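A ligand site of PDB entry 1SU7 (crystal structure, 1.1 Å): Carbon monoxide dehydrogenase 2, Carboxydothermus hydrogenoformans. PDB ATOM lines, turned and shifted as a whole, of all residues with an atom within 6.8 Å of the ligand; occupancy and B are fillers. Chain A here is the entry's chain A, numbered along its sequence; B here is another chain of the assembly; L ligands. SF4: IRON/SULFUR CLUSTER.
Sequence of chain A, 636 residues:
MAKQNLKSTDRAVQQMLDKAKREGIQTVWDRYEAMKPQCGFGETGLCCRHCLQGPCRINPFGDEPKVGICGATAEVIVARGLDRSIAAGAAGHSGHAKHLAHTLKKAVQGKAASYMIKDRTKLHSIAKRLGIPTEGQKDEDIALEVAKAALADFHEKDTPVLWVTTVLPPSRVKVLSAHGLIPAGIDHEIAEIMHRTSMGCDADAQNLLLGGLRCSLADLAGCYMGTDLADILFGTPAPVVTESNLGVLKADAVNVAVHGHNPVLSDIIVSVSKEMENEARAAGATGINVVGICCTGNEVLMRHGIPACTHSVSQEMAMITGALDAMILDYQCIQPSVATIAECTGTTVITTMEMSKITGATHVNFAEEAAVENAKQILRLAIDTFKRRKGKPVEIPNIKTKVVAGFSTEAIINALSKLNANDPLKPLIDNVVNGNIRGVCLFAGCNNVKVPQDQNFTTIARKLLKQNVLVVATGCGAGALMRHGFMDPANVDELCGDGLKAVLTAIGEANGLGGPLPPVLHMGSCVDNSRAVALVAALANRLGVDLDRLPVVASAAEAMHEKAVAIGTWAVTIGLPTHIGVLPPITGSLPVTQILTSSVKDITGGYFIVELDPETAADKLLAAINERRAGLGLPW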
ATOM      1  N   CYS A  47     -17.106  14.647  -7.014  1.00  0.00           N
ATOM      2  CA  CYS A  47     -17.463  13.482  -6.209  1.00  0.00           C
ATOM      3  C   CYS A  47     -17.040  13.812  -4.802  1.00  0.00           C
ATOM      4  O   CYS A  47     -15.976  14.387  -4.594  1.00  0.00           O
ATOM      5  CB  CYS A  47     -16.741  12.206  -6.697  1.00  0.00           C
ATOM      6  SG  CYS A  47     -17.140  10.810  -5.597  1.00  0.00           S
ATOM      7  N   CYS A  48     -17.888  13.431  -3.879  1.00  0.00           N
ATOM      8  CA  CYS A  48     -17.599  13.619  -2.450  1.00  0.00           C
ATOM      9  C   CYS A  48     -17.975  12.333  -1.703  1.00  0.00           C
ATOM     10  O   CYS A  48     -19.070  11.829  -1.858  1.00  0.00           O
ATOM     11  CB  CYS A  48     -18.431  14.777  -1.916  1.00  0.00           C
ATOM     12  SG  CYS A  48     -18.114  15.080  -0.167  1.00  0.00           S
ATOM     13  N   ARG A  49     -17.059  11.908  -0.842  1.00  0.00           N
ATOM     14  CA  ARG A  49     -17.268  10.779   0.053  1.00  0.00           C
ATOM     15  C   ARG A  49     -16.954  11.203   1.464  1.00  0.00           C
ATOM     16  O   ARG A  49     -16.535  10.381   2.257  1.00  0.00           O
ATOM     17  CB  ARG A  49     -16.354   9.605  -0.359  1.00  0.00           C
ATOM     18  CG  ARG A  49     -16.774   9.092  -1.702  1.00  0.00           C
ATOM     19  CD  ARG A  49     -15.765   8.115  -2.255  1.00  0.00           C
ATOM     20  NE  ARG A  49     -15.441   7.067  -1.372  1.00  0.00           N
ATOM     21  CZ  ARG A  49     -14.435   6.295  -1.148  1.00  0.00           C
ATOM     22  NH1 ARG A  49     -13.371   6.368  -1.911  1.00  0.00           N
ATOM     23  NH2 ARG A  49     -14.565   5.408  -0.166  1.00  0.00           N
ATOM     24  N   HIS A  50     -17.220  12.472   1.760  1.00  0.00           N
ATOM     25  CA  HIS A  50     -16.875  12.935   3.102  1.00  0.00           C
ATOM     26  C   HIS A  50     -17.850  12.508   4.167  1.00  0.00           C
ATOM     27  O   HIS A  50     -17.588  12.809   5.318  1.00  0.00           O
ATOM     28  CB  HIS A  50     -16.650  14.432   3.142  1.00  0.00           C
ATOM     29  CG  HIS A  50     -15.447  14.824   2.291  1.00  0.00           C
ATOM     30  ND1 HIS A  50     -14.915  16.059   2.429  1.00  0.00           N
ATOM     31  CD2 HIS A  50     -14.709  14.163   1.361  1.00  0.00           C
ATOM     32  CE1 HIS A  50     -13.881  16.185   1.580  1.00  0.00           C
ATOM     33  NE2 HIS A  50     -13.717  15.051   0.929  1.00  0.00           N
ATOM     34  N   CYS A  51     -18.953  11.860   3.850  1.00  0.00           N
ATOM     35  CA  CYS A  51     -19.752  11.276   4.935  1.00  0.00           C
ATOM     36  C   CYS A  51     -20.420  10.035   4.418  1.00  0.00           C
ATOM     37  O   CYS A  51     -20.368   9.773   3.234  1.00  0.00           O
ATOM     38  CB  CYS A  51     -20.797  12.258   5.524  1.00  0.00           C
ATOM     39  SG  CYS A  51     -22.252  12.528   4.517  1.00  0.00           S
ATOM     40  N   LEU A  52     -21.080   9.338   5.326  1.00  0.00           N
ATOM     41  CA  LEU A  52     -21.680   8.062   5.004  1.00  0.00           C
ATOM     42  C   LEU A  52     -23.043   8.212   4.365  1.00  0.00           C
ATOM     43  O   LEU A  52     -23.684   7.205   4.097  1.00  0.00           O
ATOM     44  CB  LEU A  52     -21.801   7.195   6.262  1.00  0.00           C
ATOM     45  CG  LEU A  52     -20.440   6.884   6.904  1.00  0.00           C
ATOM     46  CD1 LEU A  52     -20.719   6.118   8.199  1.00  0.00           C
ATOM     47  CD2 LEU A  52     -19.504   6.171   5.951  1.00  0.00           C
ATOM     48  N   GLN A  53     -23.462   9.457   4.051  1.00  0.00           N
ATOM     49  CA  GLN A  53     -24.583   9.613   3.168  1.00  0.00           C
ATOM     50  C   GLN A  53     -24.195   9.530   1.719  1.00  0.00           C
ATOM     51  O   GLN A  53     -25.010   9.326   0.850  1.00  0.00           O
ATOM     52  CB  GLN A  53     -25.310  10.967   3.367  1.00  0.00           C
ATOM     53  CG  GLN A  53     -25.912  10.982   4.752  1.00  0.00           C
ATOM     54  CD  GLN A  53     -26.584  12.287   5.137  1.00  0.00           C
ATOM     55  OE1 GLN A  53     -27.592  12.264   5.808  1.00  0.00           O
ATOM     56  NE2 GLN A  53     -26.008  13.433   4.742  1.00  0.00           N
ATOM     57  N   GLY A  54     -22.904   9.662   1.481  1.00  0.00           N
ATOM     58  CA  GLY A  54     -22.363   9.567   0.166  1.00  0.00           C
ATOM     59  C   GLY A  54     -22.214   8.114  -0.299  1.00  0.00           C
ATOM     60  O   GLY A  54     -22.637   7.180   0.385  1.00  0.00           O
ATOM     61  N   PRO A  55     -21.605   7.908  -1.446  1.00  0.00           N
ATOM     62  CA  PRO A  55     -20.948   8.937  -2.253  1.00  0.00           C
ATOM     63  C   PRO A  55     -21.939   9.863  -2.980  1.00  0.00           C
ATOM     64  O   PRO A  55     -23.005   9.434  -3.394  1.00  0.00           O
ATOM     65  CB  PRO A  55     -20.153   8.099  -3.268  1.00  0.00           C
ATOM     66  CG  PRO A  55     -20.857   6.796  -3.315  1.00  0.00           C
ATOM     67  CD  PRO A  55     -21.468   6.546  -1.989  1.00  0.00           C
ATOM     68  N   CYS A  56     -21.540  11.114  -2.994  1.00  0.00           N
ATOM     69  CA  CYS A  56     -22.266  12.100  -3.755  1.00  0.00           C
ATOM     70  C   CYS A  56     -21.484  12.428  -4.977  1.00  0.00           C
ATOM     71  O   CYS A  56     -20.261  12.454  -4.965  1.00  0.00           O
ATOM     72  CB  CYS A  56     -22.479  13.378  -2.956  1.00  0.00           C
ATOM     73  SG  CYS A  56     -23.694  13.102  -1.607  1.00  0.00           S
ATOM     74  N   ARG A  57     -22.172  12.685  -6.050  1.00  0.00           N
ATOM     75  CA  ARG A  57     -21.517  13.175  -7.276  1.00  0.00           C
ATOM     76  C   ARG A  57     -22.450  14.181  -7.859  1.00  0.00           C
ATOM     77  O   ARG A  57     -23.619  14.299  -7.502  1.00  0.00           O
ATOM     78  CB  ARG A  57     -21.273  11.984  -8.169  1.00  0.00           C
ATOM     79  CG  ARG A  57     -22.599  11.481  -8.730  1.00  0.00           C
ATOM     80  CD  ARG A  57     -22.557  10.108  -9.372  1.00  0.00           C
ATOM     81  NE  ARG A  57     -23.926   9.907  -9.989  1.00  0.00           N
ATOM     82  CZ  ARG A  57     -24.993   9.607  -9.202  1.00  0.00           C
ATOM     83  NH1 ARG A  57     -26.172   9.481  -9.875  1.00  0.00           N
ATOM     84  NH2 ARG A  57     -25.009   9.385  -7.853  1.00  0.00           N
ATOM     85  N   VAL A  67     -26.297  18.743  -6.846  1.00  0.00           N
ATOM     86  CA  VAL A  67     -25.844  19.217  -5.548  1.00  0.00           C
ATOM     87  C   VAL A  67     -25.691  17.998  -4.682  1.00  0.00           C
ATOM     88  O   VAL A  67     -26.372  16.974  -4.845  1.00  0.00           O
ATOM     89  CB  VAL A  67     -26.896  20.231  -5.008  1.00  0.00           C
ATOM     90  CG1 VAL A  67     -28.255  19.590  -4.891  1.00  0.00           C
ATOM     91  CG2 VAL A  67     -26.435  20.827  -3.723  1.00  0.00           C
ATOM     92  N   GLY A  68     -24.772  18.049  -3.744  1.00  0.00           N
ATOM     93  CA  GLY A  68     -24.599  16.980  -2.769  1.00  0.00           C
ATOM     94  C   GLY A  68     -25.802  16.842  -1.859  1.00  0.00           C
ATOM     95  O   GLY A  68     -26.605  17.755  -1.688  1.00  0.00           O
ATOM     96  N   ILE A  69     -25.861  15.701  -1.213  1.00  0.00           N
ATOM     97  CA  ILE A  69     -27.045  15.414  -0.375  1.00  0.00           C
ATOM     98  C   ILE A  69     -27.179  16.410   0.724  1.00  0.00           C
ATOM     99  O   ILE A  69     -28.284  16.825   1.043  1.00  0.00           O
ATOM    100  CB  ILE A  69     -26.926  13.985   0.169  1.00  0.00           C
ATOM    101  CG1 ILE A  69     -27.246  13.019  -1.005  1.00  0.00           C
ATOM    102  CG2 ILE A  69     -27.850  13.759   1.322  1.00  0.00           C
ATOM    103  CD1 ILE A  69     -26.883  11.616  -0.663  1.00  0.00           C
ATOM    104  N   CYS A  70     -26.068  16.859   1.335  1.00  0.00           N
ATOM    105  CA  CYS A  70     -26.160  17.845   2.394  1.00  0.00           C
ATOM    106  C   CYS A  70     -26.334  19.250   1.890  1.00  0.00           C
ATOM    107  O   CYS A  70     -26.464  20.171   2.717  1.00  0.00           O
ATOM    108  CB  CYS A  70     -24.853  17.755   3.190  1.00  0.00           C
ATOM    109  SG  CYS A  70     -23.427  18.162   2.130  1.00  0.00           S
ATOM    110  N   GLY A  71     -26.345  19.444   0.561  1.00  0.00           N
ATOM    111  CA  GLY A  71     -26.428  20.772  -0.037  1.00  0.00           C
ATOM    112  C   GLY A  71     -25.096  21.282  -0.509  1.00  0.00           C
ATOM    113  O   GLY A  71     -25.031  22.382  -1.019  1.00  0.00           O
ATOM    114  N   ALA A  72     -24.033  20.457  -0.418  1.00  0.00           N
ATOM    115  CA  ALA A  72     -22.722  20.921  -0.891  1.00  0.00           C
ATOM    116  C   ALA A  72     -22.785  21.124  -2.387  1.00  0.00           C
ATOM    117  O   ALA A  72     -23.150  20.228  -3.137  1.00  0.00           O
ATOM    118  CB  ALA A  72     -21.671  19.901  -0.494  1.00  0.00           C
ATOM    119  N   THR A  73     -22.413  22.327  -2.824  1.00  0.00           N
ATOM    120  CA  THR A  73     -22.421  22.622  -4.246  1.00  0.00           C
ATOM    121  C   THR A  73     -21.189  22.091  -4.919  1.00  0.00           C
ATOM    122  O   THR A  73     -20.218  21.647  -4.301  1.00  0.00           O
ATOM    123  CB  THR A  73     -22.438  24.134  -4.452  1.00  0.00           C
ATOM    124  OG1 THR A  73     -21.244  24.633  -3.819  1.00  0.00           O
ATOM    125  CG2 THR A  73     -23.663  24.801  -3.827  1.00  0.00           C
ATOM    126  N   ILE A  77     -17.657  21.110  -3.184  1.00  0.00           N
ATOM    127  CA  ILE A  77     -17.081  19.778  -3.272  1.00  0.00           C
ATOM    128  C   ILE A  77     -15.714  19.818  -3.945  1.00  0.00           C
ATOM    129  O   ILE A  77     -14.754  19.217  -3.439  1.00  0.00           O
ATOM    130  CB  ILE A  77     -18.047  18.868  -4.048  1.00  0.00           C
ATOM    131  CG1 ILE A  77     -19.254  18.572  -3.149  1.00  0.00           C
ATOM    132  CG2 ILE A  77     -17.356  17.615  -4.525  1.00  0.00           C
ATOM    133  CD1 ILE A  77     -20.327  17.790  -3.911  1.00  0.00           C
ATOM    134  N   ARG A  80     -13.229  21.415  -1.519  1.00  0.00           N
ATOM    135  CA  ARG A  80     -12.916  20.567  -0.384  1.00  0.00           C
ATOM    136  C   ARG A  80     -11.993  19.457  -0.795  1.00  0.00           C
ATOM    137  O   ARG A  80     -11.040  19.148  -0.073  1.00  0.00           O
ATOM    138  CB  ARG A  80     -14.206  19.954   0.202  1.00  0.00           C
ATOM    139  CG  ARG A  80     -15.053  21.021   0.886  1.00  0.00           C
ATOM    140  CD  ARG A  80     -16.155  20.446   1.784  1.00  0.00           C
ATOM    141  NE  ARG A  80     -16.964  19.484   1.015  1.00  0.00           N
ATOM    142  CZ  ARG A  80     -18.140  19.076   1.496  1.00  0.00           C
ATOM    143  NH1 ARG A  80     -18.619  19.570   2.630  1.00  0.00           N
ATOM    144  NH2 ARG A  80     -18.850  18.188   0.818  1.00  0.00           N
ATOM    145  N   THR A 197     -13.129  20.772   5.820  1.00  0.00           N
ATOM    146  CA  THR A 197     -13.627  20.091   4.645  1.00  0.00           C
ATOM    147  C   THR A 197     -14.510  18.903   4.989  1.00  0.00           C
ATOM    148  O   THR A 197     -15.051  18.283   4.080  1.00  0.00           O
ATOM    149  CB  THR A 197     -12.479  19.600   3.760  1.00  0.00           C
ATOM    150  OG1 THR A 197     -11.652  18.723   4.540  1.00  0.00           O
ATOM    151  CG2 THR A 197     -11.658  20.745   3.215  1.00  0.00           C
ATOM    152  N   SER A 198     -14.667  18.612   6.262  1.00  0.00           N
ATOM    153  CA  SER A 198     -15.582  17.539   6.677  1.00  0.00           C
ATOM    154  C   SER A 198     -17.013  18.046   6.533  1.00  0.00           C
ATOM    155  O   SER A 198     -17.295  19.222   6.275  1.00  0.00           O
ATOM    156  CB  SER A 198     -15.219  17.086   8.084  1.00  0.00           C
ATOM    157  OG  SER A 198     -15.598  17.982   9.062  1.00  0.00           O
ATOM    158  N   MET A 199     -17.930  17.096   6.648  1.00  0.00           N
ATOM    159  CA  MET A 199     -19.323  17.408   6.322  1.00  0.00           C
ATOM    160  C   MET A 199     -19.831  18.533   7.225  1.00  0.00           C
ATOM    161  O   MET A 199     -19.644  18.557   8.450  1.00  0.00           O
ATOM    162  CB  MET A 199     -20.140  16.110   6.420  1.00  0.00           C
ATOM    163  CG  MET A 199     -21.623  16.347   6.104  1.00  0.00           C
ATOM    164  SD  MET A 199     -22.534  16.948   7.549  1.00  0.00           S
ATOM    165  CE  MET A 199     -24.183  16.823   6.855  1.00  0.00           C
ATOM    166  N   GLY A 200     -20.551  19.452   6.586  1.00  0.00           N
ATOM    167  CA  GLY A 200     -21.283  20.447   7.343  1.00  0.00           C
ATOM    168  C   GLY A 200     -20.430  21.550   7.943  1.00  0.00           C
ATOM    169  O   GLY A 200     -20.867  22.172   8.889  1.00  0.00           O
ATOM    170  N   VAL B  28     -33.020  17.684   2.143  1.00  0.00           N
ATOM    171  CA  VAL B  28     -32.004  16.615   2.098  1.00  0.00           C
ATOM    172  C   VAL B  28     -32.555  15.332   1.559  1.00  0.00           C
ATOM    173  O   VAL B  28     -31.814  14.649   0.836  1.00  0.00           O
ATOM    174  CB  VAL B  28     -31.481  16.422   3.524  1.00  0.00           C
ATOM    175  CG1 VAL B  28     -32.548  15.926   4.504  1.00  0.00           C
ATOM    176  CG2 VAL B  28     -30.267  15.490   3.534  1.00  0.00           C
ATOM    177  N   MET B  35     -29.749  11.685  -5.960  1.00  0.00           N
ATOM    178  CA  MET B  35     -28.439  11.086  -6.042  1.00  0.00           C
ATOM    179  C   MET B  35     -28.493   9.617  -6.353  1.00  0.00           C
ATOM    180  O   MET B  35     -27.463   9.031  -6.638  1.00  0.00           O
ATOM    181  CB  MET B  35     -27.791  11.305  -4.648  1.00  0.00           C
ATOM    182  CG  MET B  35     -26.272  11.111  -4.725  1.00  0.00           C
ATOM    183  SD  MET B  35     -25.450  12.276  -5.826  1.00  0.00           S
ATOM    184  CE  MET B  35     -25.716  13.836  -4.997  1.00  0.00           C
ATOM    185  N   GLN B  38     -26.565   5.548  -6.032  1.00  0.00           N
ATOM    186  CA  GLN B  38     -25.233   6.047  -5.671  1.00  0.00           C
ATOM    187  C   GLN B  38     -24.165   5.120  -6.198  1.00  0.00           C
ATOM    188  O   GLN B  38     -24.367   3.962  -6.480  1.00  0.00           O
ATOM    189  CB  GLN B  38     -25.164   6.186  -4.139  1.00  0.00           C
ATOM    190  CG  GLN B  38     -26.075   7.337  -3.705  1.00  0.00           C
ATOM    191  CD  GLN B  38     -25.994   7.579  -2.207  1.00  0.00           C
ATOM    192  OE1 GLN B  38     -25.261   8.485  -1.795  1.00  0.00           O
ATOM    193  NE2 GLN B  38     -26.694   6.824  -1.441  1.00  0.00           N
ATOM    194  N   PRO B 336     -25.160  22.710   4.317  1.00  0.00           N
ATOM    195  CA  PRO B 336     -25.035  24.072   3.725  1.00  0.00           C
ATOM    196  C   PRO B 336     -26.276  24.463   2.930  1.00  0.00           C
ATOM    197  O   PRO B 336     -26.423  25.646   2.637  1.00  0.00           O
ATOM    198  CB  PRO B 336     -23.788  23.935   2.856  1.00  0.00           C
ATOM    199  CG  PRO B 336     -23.679  22.467   2.534  1.00  0.00           C
ATOM    200  CD  PRO B 336     -24.104  21.776   3.842  1.00  0.00           C
ATOM    201  N   MET B 560     -23.284   8.959  10.196  1.00  0.00           N
ATOM    202  CA  MET B 560     -23.103   9.765   8.979  1.00  0.00           C
ATOM    203  C   MET B 560     -21.699  10.335   8.918  1.00  0.00           C
ATOM    204  O   MET B 560     -20.995  10.176   7.945  1.00  0.00           O
ATOM    205  CB  MET B 560     -24.186  10.851   8.944  1.00  0.00           C
ATOM    206  CG  MET B 560     -24.067  11.799   7.765  1.00  0.00           C
ATOM    207  SD  MET B 560     -23.124  13.305   8.070  1.00  0.00           S
ATOM    208  CE  MET B 560     -24.048  14.055   9.423  1.00  0.00           C
HETATM  209 FE1  SF4 L   1     -22.346  16.217   1.642  1.00  0.00          FE
HETATM  210 FE2  SF4 L   1     -20.174  14.852   0.767  1.00  0.00          FE
HETATM  211 FE3  SF4 L   1     -22.581  13.955   0.157  1.00  0.00          FE
HETATM  212 FE4  SF4 L   1     -21.706  13.718   2.684  1.00  0.00          FE
HETATM  213  S1  SF4 L   1     -20.825  12.670   0.914  1.00  0.00           S
HETATM  214  S2  SF4 L   1     -23.784  14.436   1.980  1.00  0.00           S
HETATM  215  S3  SF4 L   1     -20.453  15.652   2.828  1.00  0.00           S
HETATM  216  S4  SF4 L   1     -21.698  16.004  -0.489  1.00  0.00           S
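The backbone NH (N) of Gln 53 lies close to the side-chain sulfur (SG) of Cys 51 (3.3 Å).
The backbone carbonyl oxygen of Cys 56 is in hydrogen-bond range of the backbone NH of Cys 48 (2.8 Å).
N of Ile 69 lies close to SG of Cys 56, 3.4 Å away.
The side-chain sulfur (SG) of Cys 47 sits close to the backbone carbonyl oxygen (O) of Cys 56 (3.6 Å).
SG of Cys 48 lies close to NH2 of Arg 80 (3.3 Å).
The side-chain sulfur (SG) of Cys 48 sits close to the backbone NH (N) of His 50, 3.4 Å away.
SG of Cys 70 lies close to N of Ala 72 (3.5 Å).
A ring nitrogen (ND1) of His 50 lies within hydrogen-bond range of the backbone carbonyl oxygen of Thr 197.
A sulfur (S1) of the ligand lies close to the backbone NH (N) of Cys 51.
FE4 of the ligand is bound by SG of Cys 51.
The side-chain sulfur (SG) of Cys 56 is bound to an iron atom (FE3) of the ligand.
FE2 of the ligand is bound by SG of Cys 48 (2.3 Å).
A sulfur (S2) of the ligand lies close to the backbone NH (N) of Cys 70, 3.4 Å away.
SG of Cys 70 is bound to FE1 of the ligand, at 2.3 Å.
A sulfur (S1) of the ligand sits close to the backbone NH (N) of Gly 54, 3.7 Å away.
NH2 of Arg 80 sits close to S3 of the ligand.
The side-chain amide nitrogen (NE2) of Gln 53 lies close to a sulfur (S2) of the ligand (3.7 Å).
A sulfur (S1) of the ligand lies close to the backbone NH (N) of His 50 (3.7 Å).
Gly 68 touches the ligand.
Ile 69 touches the ligand (CB to S2, 3.7 Å).
Ala 72 touches the ligand (CB to S4, 3.9 Å).
Met 199 touches the ligand (CG to S3, 3.5 Å).
Along chain A the residues within 4 Å of the ligand span positions 48 to 199.
The nearest printed residue that does not touch the ligand is Ile 77 (4.1 Å).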
